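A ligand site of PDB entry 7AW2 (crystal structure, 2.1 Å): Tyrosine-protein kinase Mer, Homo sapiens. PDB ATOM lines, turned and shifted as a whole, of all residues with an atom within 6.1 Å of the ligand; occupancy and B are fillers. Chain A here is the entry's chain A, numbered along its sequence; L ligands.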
ATOM      1  N   LEU A  27     -23.545   4.108 -15.673  1.00  0.00           N
ATOM      2  CA  LEU A  27     -22.254   4.288 -16.364  1.00  0.00           C
ATOM      3  C   LEU A  27     -22.087   5.732 -16.877  1.00  0.00           C
ATOM      4  O   LEU A  27     -20.956   6.215 -16.971  1.00  0.00           O
ATOM      5  CB  LEU A  27     -22.100   3.297 -17.531  1.00  0.00           C
ATOM      6  CG  LEU A  27     -22.182   1.799 -17.221  1.00  0.00           C
ATOM      7  CD1 LEU A  27     -22.396   0.995 -18.493  1.00  0.00           C
ATOM      8  CD2 LEU A  27     -20.953   1.318 -16.482  1.00  0.00           C
ATOM      9  N   VAL A  35     -27.015   5.695 -19.308  1.00  0.00           N
ATOM     10  CA  VAL A  35     -26.409   4.439 -19.739  1.00  0.00           C
ATOM     11  C   VAL A  35     -26.142   3.672 -18.430  1.00  0.00           C
ATOM     12  O   VAL A  35     -25.545   4.229 -17.507  1.00  0.00           O
ATOM     13  CB  VAL A  35     -25.117   4.601 -20.588  1.00  0.00           C
ATOM     14  CG1 VAL A  35     -24.590   3.233 -21.051  1.00  0.00           C
ATOM     15  CG2 VAL A  35     -25.344   5.517 -21.791  1.00  0.00           C
ATOM     16  N   VAL A  50     -25.302  -6.757 -20.407  1.00  0.00           N
ATOM     17  CA  VAL A  50     -25.807  -5.805 -21.402  1.00  0.00           C
ATOM     18  C   VAL A  50     -25.573  -4.349 -20.964  1.00  0.00           C
ATOM     19  O   VAL A  50     -25.318  -4.079 -19.802  1.00  0.00           O
ATOM     20  CB  VAL A  50     -27.317  -6.048 -21.763  1.00  0.00           C
ATOM     21  CG1 VAL A  50     -27.529  -7.418 -22.424  1.00  0.00           C
ATOM     22  CG2 VAL A  50     -28.239  -5.875 -20.546  1.00  0.00           C
ATOM     23  N   ALA A  51     -25.661  -3.417 -21.937  1.00  0.00           N
ATOM     24  CA  ALA A  51     -25.661  -1.986 -21.722  1.00  0.00           C
ATOM     25  C   ALA A  51     -27.127  -1.562 -21.924  1.00  0.00           C
ATOM     26  O   ALA A  51     -27.763  -2.025 -22.863  1.00  0.00           O
ATOM     27  CB  ALA A  51     -24.758  -1.287 -22.724  1.00  0.00           C
ATOM     28  N   VAL A  52     -27.675  -0.788 -20.990  1.00  0.00           N
ATOM     29  CA  VAL A  52     -29.067  -0.333 -21.003  1.00  0.00           C
ATOM     30  C   VAL A  52     -29.118   1.195 -21.116  1.00  0.00           C
ATOM     31  O   VAL A  52     -28.684   1.896 -20.204  1.00  0.00           O
ATOM     32  CB  VAL A  52     -29.856  -0.859 -19.771  1.00  0.00           C
ATOM     33  CG1 VAL A  52     -31.325  -0.416 -19.824  1.00  0.00           C
ATOM     34  CG2 VAL A  52     -29.736  -2.374 -19.647  1.00  0.00           C
ATOM     35  N   LYS A  53     -29.644   1.695 -22.251  1.00  0.00           N
ATOM     36  CA  LYS A  53     -29.818   3.129 -22.528  1.00  0.00           C
ATOM     37  C   LYS A  53     -31.259   3.554 -22.236  1.00  0.00           C
ATOM     38  O   LYS A  53     -32.173   3.071 -22.874  1.00  0.00           O
ATOM     39  CB  LYS A  53     -29.389   3.468 -23.972  1.00  0.00           C
ATOM     40  CG  LYS A  53     -29.752   4.904 -24.443  1.00  0.00           C
ATOM     41  CD  LYS A  53     -28.932   5.985 -23.751  1.00  0.00           C
ATOM     42  CE  LYS A  53     -29.231   7.359 -24.295  1.00  0.00           C
ATOM     43  NZ  LYS A  53     -28.154   8.323 -23.932  1.00  0.00           N
ATOM     44  N   MET A  55     -34.316   6.480 -21.984  1.00  0.00           N
ATOM     45  CA  MET A  55     -34.654   7.680 -22.740  1.00  0.00           C
ATOM     46  C   MET A  55     -35.857   8.447 -22.176  1.00  0.00           C
ATOM     47  O   MET A  55     -36.508   7.978 -21.233  1.00  0.00           O
ATOM     48  CB  MET A  55     -34.828   7.333 -24.231  1.00  0.00           C
ATOM     49  CG  MET A  55     -33.483   7.088 -24.908  1.00  0.00           C
ATOM     50  SD  MET A  55     -33.569   6.274 -26.500  1.00  0.00           S
ATOM     51  CE  MET A  55     -33.879   7.661 -27.551  1.00  0.00           C
ATOM     52  N   GLU A  67     -43.617   5.748 -31.639  1.00  0.00           N
ATOM     53  CA  GLU A  67     -42.548   6.188 -32.540  1.00  0.00           C
ATOM     54  C   GLU A  67     -41.243   5.531 -32.130  1.00  0.00           C
ATOM     55  O   GLU A  67     -40.482   5.109 -33.003  1.00  0.00           O
ATOM     56  CB  GLU A  67     -42.412   7.726 -32.478  1.00  0.00           C
ATOM     57  CG  GLU A  67     -41.783   8.350 -33.713  1.00  0.00           C
ATOM     58  CD  GLU A  67     -41.926   9.864 -33.757  1.00  0.00           C
ATOM     59  OE1 GLU A  67     -42.695  10.356 -34.612  1.00  0.00           O
ATOM     60  OE2 GLU A  67     -41.281  10.553 -32.939  1.00  0.00           O
ATOM     61  N   PHE A  68     -40.995   5.422 -30.808  1.00  0.00           N
ATOM     62  CA  PHE A  68     -39.804   4.792 -30.249  1.00  0.00           C
ATOM     63  C   PHE A  68     -39.811   3.294 -30.598  1.00  0.00           C
ATOM     64  O   PHE A  68     -38.808   2.780 -31.065  1.00  0.00           O
ATOM     65  CB  PHE A  68     -39.711   5.017 -28.706  1.00  0.00           C
ATOM     66  CG  PHE A  68     -38.791   4.058 -27.981  1.00  0.00           C
ATOM     67  CD1 PHE A  68     -37.412   4.252 -27.999  1.00  0.00           C
ATOM     68  CD2 PHE A  68     -39.303   2.929 -27.336  1.00  0.00           C
ATOM     69  CE1 PHE A  68     -36.559   3.349 -27.357  1.00  0.00           C
ATOM     70  CE2 PHE A  68     -38.439   2.017 -26.718  1.00  0.00           C
ATOM     71  CZ  PHE A  68     -37.080   2.247 -26.709  1.00  0.00           C
ATOM     72  N   LEU A  69     -40.955   2.619 -30.380  1.00  0.00           N
ATOM     73  CA  LEU A  69     -41.144   1.201 -30.695  1.00  0.00           C
ATOM     74  C   LEU A  69     -40.929   0.956 -32.194  1.00  0.00           C
ATOM     75  O   LEU A  69     -40.202   0.029 -32.559  1.00  0.00           O
ATOM     76  CB  LEU A  69     -42.528   0.714 -30.244  1.00  0.00           C
ATOM     77  CG  LEU A  69     -42.843   0.717 -28.742  1.00  0.00           C
ATOM     78  CD1 LEU A  69     -44.351   0.454 -28.500  1.00  0.00           C
ATOM     79  CD2 LEU A  69     -41.981  -0.298 -27.960  1.00  0.00           C
ATOM     80  N   GLU A  71     -39.229   2.901 -34.433  1.00  0.00           N
ATOM     81  CA  GLU A  71     -37.824   3.164 -34.707  1.00  0.00           C
ATOM     82  C   GLU A  71     -36.956   2.023 -34.222  1.00  0.00           C
ATOM     83  O   GLU A  71     -36.015   1.645 -34.928  1.00  0.00           O
ATOM     84  CB  GLU A  71     -37.365   4.490 -34.079  1.00  0.00           C
ATOM     85  CG  GLU A  71     -37.853   5.730 -34.821  1.00  0.00           C
ATOM     86  CD  GLU A  71     -38.056   6.985 -33.988  1.00  0.00           C
ATOM     87  OE1 GLU A  71     -37.717   6.985 -32.784  1.00  0.00           O
ATOM     88  OE2 GLU A  71     -38.571   7.980 -34.560  1.00  0.00           O
ATOM     89  N   ALA A  72     -37.250   1.479 -33.022  1.00  0.00           N
ATOM     90  CA  ALA A  72     -36.545   0.340 -32.426  1.00  0.00           C
ATOM     91  C   ALA A  72     -36.749  -0.932 -33.264  1.00  0.00           C
ATOM     92  O   ALA A  72     -35.781  -1.648 -33.507  1.00  0.00           O
ATOM     93  CB  ALA A  72     -37.013   0.108 -30.989  1.00  0.00           C
ATOM     94  N   MET A  75     -34.417  -0.692 -36.234  1.00  0.00           N
ATOM     95  CA  MET A  75     -33.067  -0.856 -35.711  1.00  0.00           C
ATOM     96  C   MET A  75     -32.677  -2.317 -35.446  1.00  0.00           C
ATOM     97  O   MET A  75     -31.559  -2.701 -35.757  1.00  0.00           O
ATOM     98  CB  MET A  75     -32.901  -0.070 -34.415  1.00  0.00           C
ATOM     99  CG  MET A  75     -31.739   0.863 -34.443  1.00  0.00           C
ATOM    100  SD  MET A  75     -32.205   2.380 -35.310  1.00  0.00           S
ATOM    101  CE  MET A  75     -32.793   3.336 -33.942  1.00  0.00           C
ATOM    102  N   ILE A  84     -23.802  -1.829 -34.405  1.00  0.00           N
ATOM    103  CA  ILE A  84     -24.206  -2.318 -33.087  1.00  0.00           C
ATOM    104  C   ILE A  84     -25.548  -3.072 -33.220  1.00  0.00           C
ATOM    105  O   ILE A  84     -26.416  -2.670 -34.016  1.00  0.00           O
ATOM    106  CB  ILE A  84     -24.245  -1.190 -32.003  1.00  0.00           C
ATOM    107  CG1 ILE A  84     -24.250  -1.790 -30.567  1.00  0.00           C
ATOM    108  CG2 ILE A  84     -25.422  -0.235 -32.193  1.00  0.00           C
ATOM    109  CD1 ILE A  84     -23.627  -0.851 -29.517  1.00  0.00           C
ATOM    110  N   LEU A  86     -29.136  -4.186 -31.829  1.00  0.00           N
ATOM    111  CA  LEU A  86     -30.117  -3.843 -30.819  1.00  0.00           C
ATOM    112  C   LEU A  86     -30.625  -5.179 -30.307  1.00  0.00           C
ATOM    113  O   LEU A  86     -31.052  -5.994 -31.119  1.00  0.00           O
ATOM    114  CB  LEU A  86     -31.269  -3.051 -31.449  1.00  0.00           C
ATOM    115  CG  LEU A  86     -32.322  -2.532 -30.476  1.00  0.00           C
ATOM    116  CD1 LEU A  86     -31.765  -1.418 -29.632  1.00  0.00           C
ATOM    117  CD2 LEU A  86     -33.521  -2.032 -31.224  1.00  0.00           C
ATOM    118  N   VAL A  89     -35.935  -3.739 -26.639  1.00  0.00           N
ATOM    119  CA  VAL A  89     -36.382  -2.548 -25.922  1.00  0.00           C
ATOM    120  C   VAL A  89     -37.315  -2.888 -24.747  1.00  0.00           C
ATOM    121  O   VAL A  89     -37.943  -3.947 -24.744  1.00  0.00           O
ATOM    122  CB  VAL A  89     -36.990  -1.450 -26.851  1.00  0.00           C
ATOM    123  CG1 VAL A  89     -35.952  -0.891 -27.823  1.00  0.00           C
ATOM    124  CG2 VAL A  89     -38.240  -1.952 -27.599  1.00  0.00           C
ATOM    125  N   VAL A 103     -33.365   0.908 -24.131  1.00  0.00           N
ATOM    126  CA  VAL A 103     -32.845   0.167 -25.285  1.00  0.00           C
ATOM    127  C   VAL A 103     -31.686  -0.698 -24.775  1.00  0.00           C
ATOM    128  O   VAL A 103     -30.870  -0.228 -23.982  1.00  0.00           O
ATOM    129  CB  VAL A 103     -32.580   0.991 -26.595  1.00  0.00           C
ATOM    130  CG1 VAL A 103     -33.098   2.421 -26.508  1.00  0.00           C
ATOM    131  CG2 VAL A 103     -31.126   0.941 -27.058  1.00  0.00           C
ATOM    132  N   LEU A 105     -28.479  -3.174 -25.331  1.00  0.00           N
ATOM    133  CA  LEU A 105     -27.355  -3.351 -26.232  1.00  0.00           C
ATOM    134  C   LEU A 105     -26.338  -4.314 -25.713  1.00  0.00           C
ATOM    135  O   LEU A 105     -26.200  -4.439 -24.495  1.00  0.00           O
ATOM    136  CB  LEU A 105     -26.692  -1.959 -26.487  1.00  0.00           C
ATOM    137  CG  LEU A 105     -27.647  -0.861 -27.031  1.00  0.00           C
ATOM    138  CD1 LEU A 105     -27.308   0.490 -26.492  1.00  0.00           C
ATOM    139  CD2 LEU A 105     -27.764  -0.881 -28.541  1.00  0.00           C
ATOM    140  N   PRO A 106     -25.504  -4.929 -26.592  1.00  0.00           N
ATOM    141  CA  PRO A 106     -24.377  -5.745 -26.081  1.00  0.00           C
ATOM    142  C   PRO A 106     -23.412  -4.873 -25.250  1.00  0.00           C
ATOM    143  O   PRO A 106     -23.214  -3.702 -25.581  1.00  0.00           O
ATOM    144  CB  PRO A 106     -23.691  -6.247 -27.362  1.00  0.00           C
ATOM    145  CG  PRO A 106     -24.636  -5.998 -28.453  1.00  0.00           C
ATOM    146  CD  PRO A 106     -25.484  -4.865 -28.067  1.00  0.00           C
ATOM    147  N   PHE A 107     -22.875  -5.425 -24.140  1.00  0.00           N
ATOM    148  CA  PHE A 107     -21.979  -4.652 -23.290  1.00  0.00           C
ATOM    149  C   PHE A 107     -20.592  -4.590 -23.930  1.00  0.00           C
ATOM    150  O   PHE A 107     -20.031  -5.615 -24.289  1.00  0.00           O
ATOM    151  CB  PHE A 107     -21.918  -5.171 -21.851  1.00  0.00           C
ATOM    152  CG  PHE A 107     -21.140  -4.275 -20.911  1.00  0.00           C
ATOM    153  CD1 PHE A 107     -21.727  -3.166 -20.322  1.00  0.00           C
ATOM    154  CD2 PHE A 107     -19.795  -4.531 -20.628  1.00  0.00           C
ATOM    155  CE1 PHE A 107     -21.009  -2.339 -19.460  1.00  0.00           C
ATOM    156  CE2 PHE A 107     -19.072  -3.708 -19.778  1.00  0.00           C
ATOM    157  CZ  PHE A 107     -19.683  -2.621 -19.193  1.00  0.00           C
ATOM    158  N   MET A 108     -20.061  -3.370 -24.098  1.00  0.00           N
ATOM    159  CA  MET A 108     -18.742  -3.160 -24.713  1.00  0.00           C
ATOM    160  C   MET A 108     -17.775  -2.602 -23.692  1.00  0.00           C
ATOM    161  O   MET A 108     -17.706  -1.376 -23.514  1.00  0.00           O
ATOM    162  CB  MET A 108     -18.822  -2.265 -25.971  1.00  0.00           C
ATOM    163  CG  MET A 108     -20.027  -2.545 -26.831  1.00  0.00           C
ATOM    164  SD  MET A 108     -19.536  -3.096 -28.472  1.00  0.00           S
ATOM    165  CE  MET A 108     -21.148  -3.464 -29.182  1.00  0.00           C
ATOM    166  N   LYS A 109     -17.044  -3.523 -23.035  1.00  0.00           N
ATOM    167  CA  LYS A 109     -16.060  -3.238 -21.995  1.00  0.00           C
ATOM    168  C   LYS A 109     -14.931  -2.285 -22.462  1.00  0.00           C
ATOM    169  O   LYS A 109     -14.454  -1.515 -21.644  1.00  0.00           O
ATOM    170  CB  LYS A 109     -15.498  -4.526 -21.349  1.00  0.00           C
ATOM    171  CG  LYS A 109     -14.549  -5.342 -22.236  1.00  0.00           C
ATOM    172  CD  LYS A 109     -13.964  -6.543 -21.512  1.00  0.00           C
ATOM    173  CE  LYS A 109     -12.943  -7.235 -22.375  1.00  0.00           C
ATOM    174  NZ  LYS A 109     -12.193  -8.275 -21.612  1.00  0.00           N
ATOM    175  N   GLY A 111     -15.327   0.241 -24.523  1.00  0.00           N
ATOM    176  CA  GLY A 111     -15.950   1.548 -24.680  1.00  0.00           C
ATOM    177  C   GLY A 111     -15.948   2.107 -26.096  1.00  0.00           C
ATOM    178  O   GLY A 111     -15.817   1.371 -27.082  1.00  0.00           O
ATOM    179  N   MET A 164     -18.215   1.950 -31.416  1.00  0.00           N
ATOM    180  CA  MET A 164     -17.906   1.146 -30.245  1.00  0.00           C
ATOM    181  C   MET A 164     -16.888   0.083 -30.575  1.00  0.00           C
ATOM    182  O   MET A 164     -16.791  -0.332 -31.720  1.00  0.00           O
ATOM    183  CB  MET A 164     -19.192   0.529 -29.639  1.00  0.00           C
ATOM    184  CG  MET A 164     -20.188   1.583 -29.108  1.00  0.00           C
ATOM    185  SD  MET A 164     -19.597   2.675 -27.743  1.00  0.00           S
ATOM    186  CE  MET A 164     -19.333   1.437 -26.371  1.00  0.00           C
ATOM    187  N   ALA A 174     -22.620   2.975 -33.965  1.00  0.00           N
ATOM    188  CA  ALA A 174     -23.614   2.920 -32.899  1.00  0.00           C
ATOM    189  C   ALA A 174     -24.202   4.292 -32.637  1.00  0.00           C
ATOM    190  O   ALA A 174     -23.934   5.223 -33.402  1.00  0.00           O
ATOM    191  CB  ALA A 174     -22.938   2.399 -31.621  1.00  0.00           C
ATOM    192  N   ASP A 175     -25.003   4.423 -31.561  1.00  0.00           N
ATOM    193  CA  ASP A 175     -25.575   5.673 -31.046  1.00  0.00           C
ATOM    194  C   ASP A 175     -26.062   6.570 -32.152  1.00  0.00           C
ATOM    195  O   ASP A 175     -25.636   7.735 -32.269  1.00  0.00           O
ATOM    196  CB  ASP A 175     -24.506   6.374 -30.198  1.00  0.00           C
ATOM    197  CG  ASP A 175     -24.898   6.652 -28.760  1.00  0.00           C
ATOM    198  OD1 ASP A 175     -26.089   6.984 -28.523  1.00  0.00           O
ATOM    199  OD2 ASP A 175     -24.030   6.562 -27.882  1.00  0.00           O
ATOM    200  N   PHE A 176     -26.949   5.993 -32.999  1.00  0.00           N
ATOM    201  CA  PHE A 176     -27.543   6.610 -34.174  1.00  0.00           C
ATOM    202  C   PHE A 176     -28.265   7.885 -33.770  1.00  0.00           C
ATOM    203  O   PHE A 176     -28.917   7.887 -32.711  1.00  0.00           O
ATOM    204  CB  PHE A 176     -28.491   5.610 -34.889  1.00  0.00           C
ATOM    205  CG  PHE A 176     -27.951   4.202 -34.981  1.00  0.00           C
ATOM    206  CD1 PHE A 176     -26.885   3.903 -35.826  1.00  0.00           C
ATOM    207  CD2 PHE A 176     -28.438   3.194 -34.153  1.00  0.00           C
ATOM    208  CE1 PHE A 176     -26.339   2.610 -35.865  1.00  0.00           C
ATOM    209  CE2 PHE A 176     -27.885   1.909 -34.183  1.00  0.00           C
ATOM    210  CZ  PHE A 176     -26.844   1.620 -35.052  1.00  0.00           C
ATOM    211  N   GLY A 177     -28.088   8.934 -34.568  1.00  0.00           N
ATOM    212  CA  GLY A 177     -28.662  10.262 -34.343  1.00  0.00           C
ATOM    213  C   GLY A 177     -30.109  10.272 -33.903  1.00  0.00           C
ATOM    214  O   GLY A 177     -30.942   9.587 -34.508  1.00  0.00           O
ATOM    215  N   LEU A 178     -30.397  11.029 -32.817  1.00  0.00           N
ATOM    216  CA  LEU A 178     -31.701  11.176 -32.145  1.00  0.00           C
ATOM    217  C   LEU A 178     -32.206   9.847 -31.560  1.00  0.00           C
ATOM    218  O   LEU A 178     -31.578   9.282 -30.665  1.00  0.00           O
ATOM    219  CB  LEU A 178     -32.761  11.849 -33.034  1.00  0.00           C
HETATM  220  C1  LIG L   1     -23.422   3.339 -26.424  1.00  0.00           C
HETATM  221  C2  LIG L   1     -22.908   2.129 -25.689  1.00  0.00           C
HETATM  222  C3  LIG L   1     -23.055   0.769 -26.192  1.00  0.00           C
HETATM  223  C4  LIG L   1     -21.156   1.130 -22.551  1.00  0.00           C
HETATM  224  C5  LIG L   1     -22.297   2.299 -24.489  1.00  0.00           C
HETATM  225  C6  LIG L   1     -25.529   3.226 -27.648  1.00  0.00           C
HETATM  226  C7  LIG L   1     -27.240   3.198 -28.905  1.00  0.00           C
HETATM  227  C8  LIG L   1     -28.632   3.453 -29.299  1.00  0.00           C
HETATM  228  C9  LIG L   1     -29.436   4.257 -28.487  1.00  0.00           C
HETATM  229  C10 LIG L   1     -30.746   4.510 -28.843  1.00  0.00           C
HETATM  230  C11 LIG L   1     -31.306   3.995 -30.015  1.00  0.00           C
HETATM  231  C12 LIG L   1     -30.482   3.204 -30.823  1.00  0.00           C
HETATM  232  C13 LIG L   1     -29.175   2.929 -30.477  1.00  0.00           C
HETATM  233  C14 LIG L   1     -34.330   6.053 -30.849  1.00  0.00           C
HETATM  234  C15 LIG L   1     -35.319   5.108 -31.071  1.00  0.00           C
HETATM  235  C16 LIG L   1     -35.021   3.762 -30.954  1.00  0.00           C
HETATM  236  C17 LIG L   1     -33.738   3.375 -30.614  1.00  0.00           C
HETATM  237 CL1  LIG L   1     -33.419   1.676 -30.481  1.00  0.00          CL
HETATM  238  C18 LIG L   1     -33.047   5.666 -30.510  1.00  0.00           C
HETATM  239  C19 LIG L   1     -32.718   4.307 -30.381  1.00  0.00           C
HETATM  240  N1  LIG L   1     -26.283   2.659 -29.589  1.00  0.00           N
HETATM  241  N2  LIG L   1     -25.146   2.667 -28.757  1.00  0.00           N
HETATM  242  O1  LIG L   1     -26.836   3.596 -27.658  1.00  0.00           O
HETATM  243  N3  LIG L   1     -24.869   3.500 -26.502  1.00  0.00           N
HETATM  244  C20 LIG L   1     -25.576   3.676 -25.234  1.00  0.00           C
HETATM  245  N4  LIG L   1     -21.814   1.215 -23.762  1.00  0.00           N
HETATM  246  C21 LIG L   1     -20.919  -0.187 -22.342  1.00  0.00           C
HETATM  247  N5  LIG L   1     -21.404  -0.934 -23.376  1.00  0.00           N
HETATM  248  C22 LIG L   1     -21.947  -0.083 -24.247  1.00  0.00           C
HETATM  249  C23 LIG L   1     -22.585  -0.301 -25.492  1.00  0.00           C
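The backbone NH of Met 108 is in hydrogen-bond range of a nitrogen (N5) of the ligand (2.9 Å). N of Asp 175 lies within hydrogen-bond range of N1 of the ligand (2.9 Å).
The backbone carbonyl oxygen (O) of Leu 105 lies within hydrogen-bond range of the backbone NH (N) of Ala 51, 2.8 Å away. O of Val 35 is in hydrogen-bond range of N of Leu 27, at 2.7 Å. N of Val 103 is in hydrogen-bond range of O of Lys 53 (2.8 Å).
Val 35 touches the ligand (CG2 to C20, 3.9 Å). Ala 51 touches the ligand (CB to C22, 3.4 Å). Met 55 touches the ligand (CE to C18, 3.7 Å). CD1 of Phe 68 touches C15 of the ligand (3.8 Å). OE1 of Glu 71 touches C15 of the ligand, 3.5 Å away. N of Ala 72 touches C16 of the ligand (3.8 Å). CE of Met 75 touches C17 of the ligand, 3.5 Å away. Ile 84 touches the ligand (CD1 to C3, 3.7 Å). Leu 86 touches the ligand (CD1 to CL1, 3.6 Å). Val 103 touches the ligand (CG1 to C10, 3.9 Å). Leu 105 touches the ligand. Pro 106 touches the ligand (O to C23, 3.5 Å). Phe 107 touches the ligand. CE of Met 164 touches N4 of the ligand, at 3.6 Å. CB of Ala 174 touches N2 of the ligand (3.6 Å). Phe 176 touches the ligand. Leu 178 touches the ligand. Along chain A the residues within 4 Å of the ligand span positions 35 to 178.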
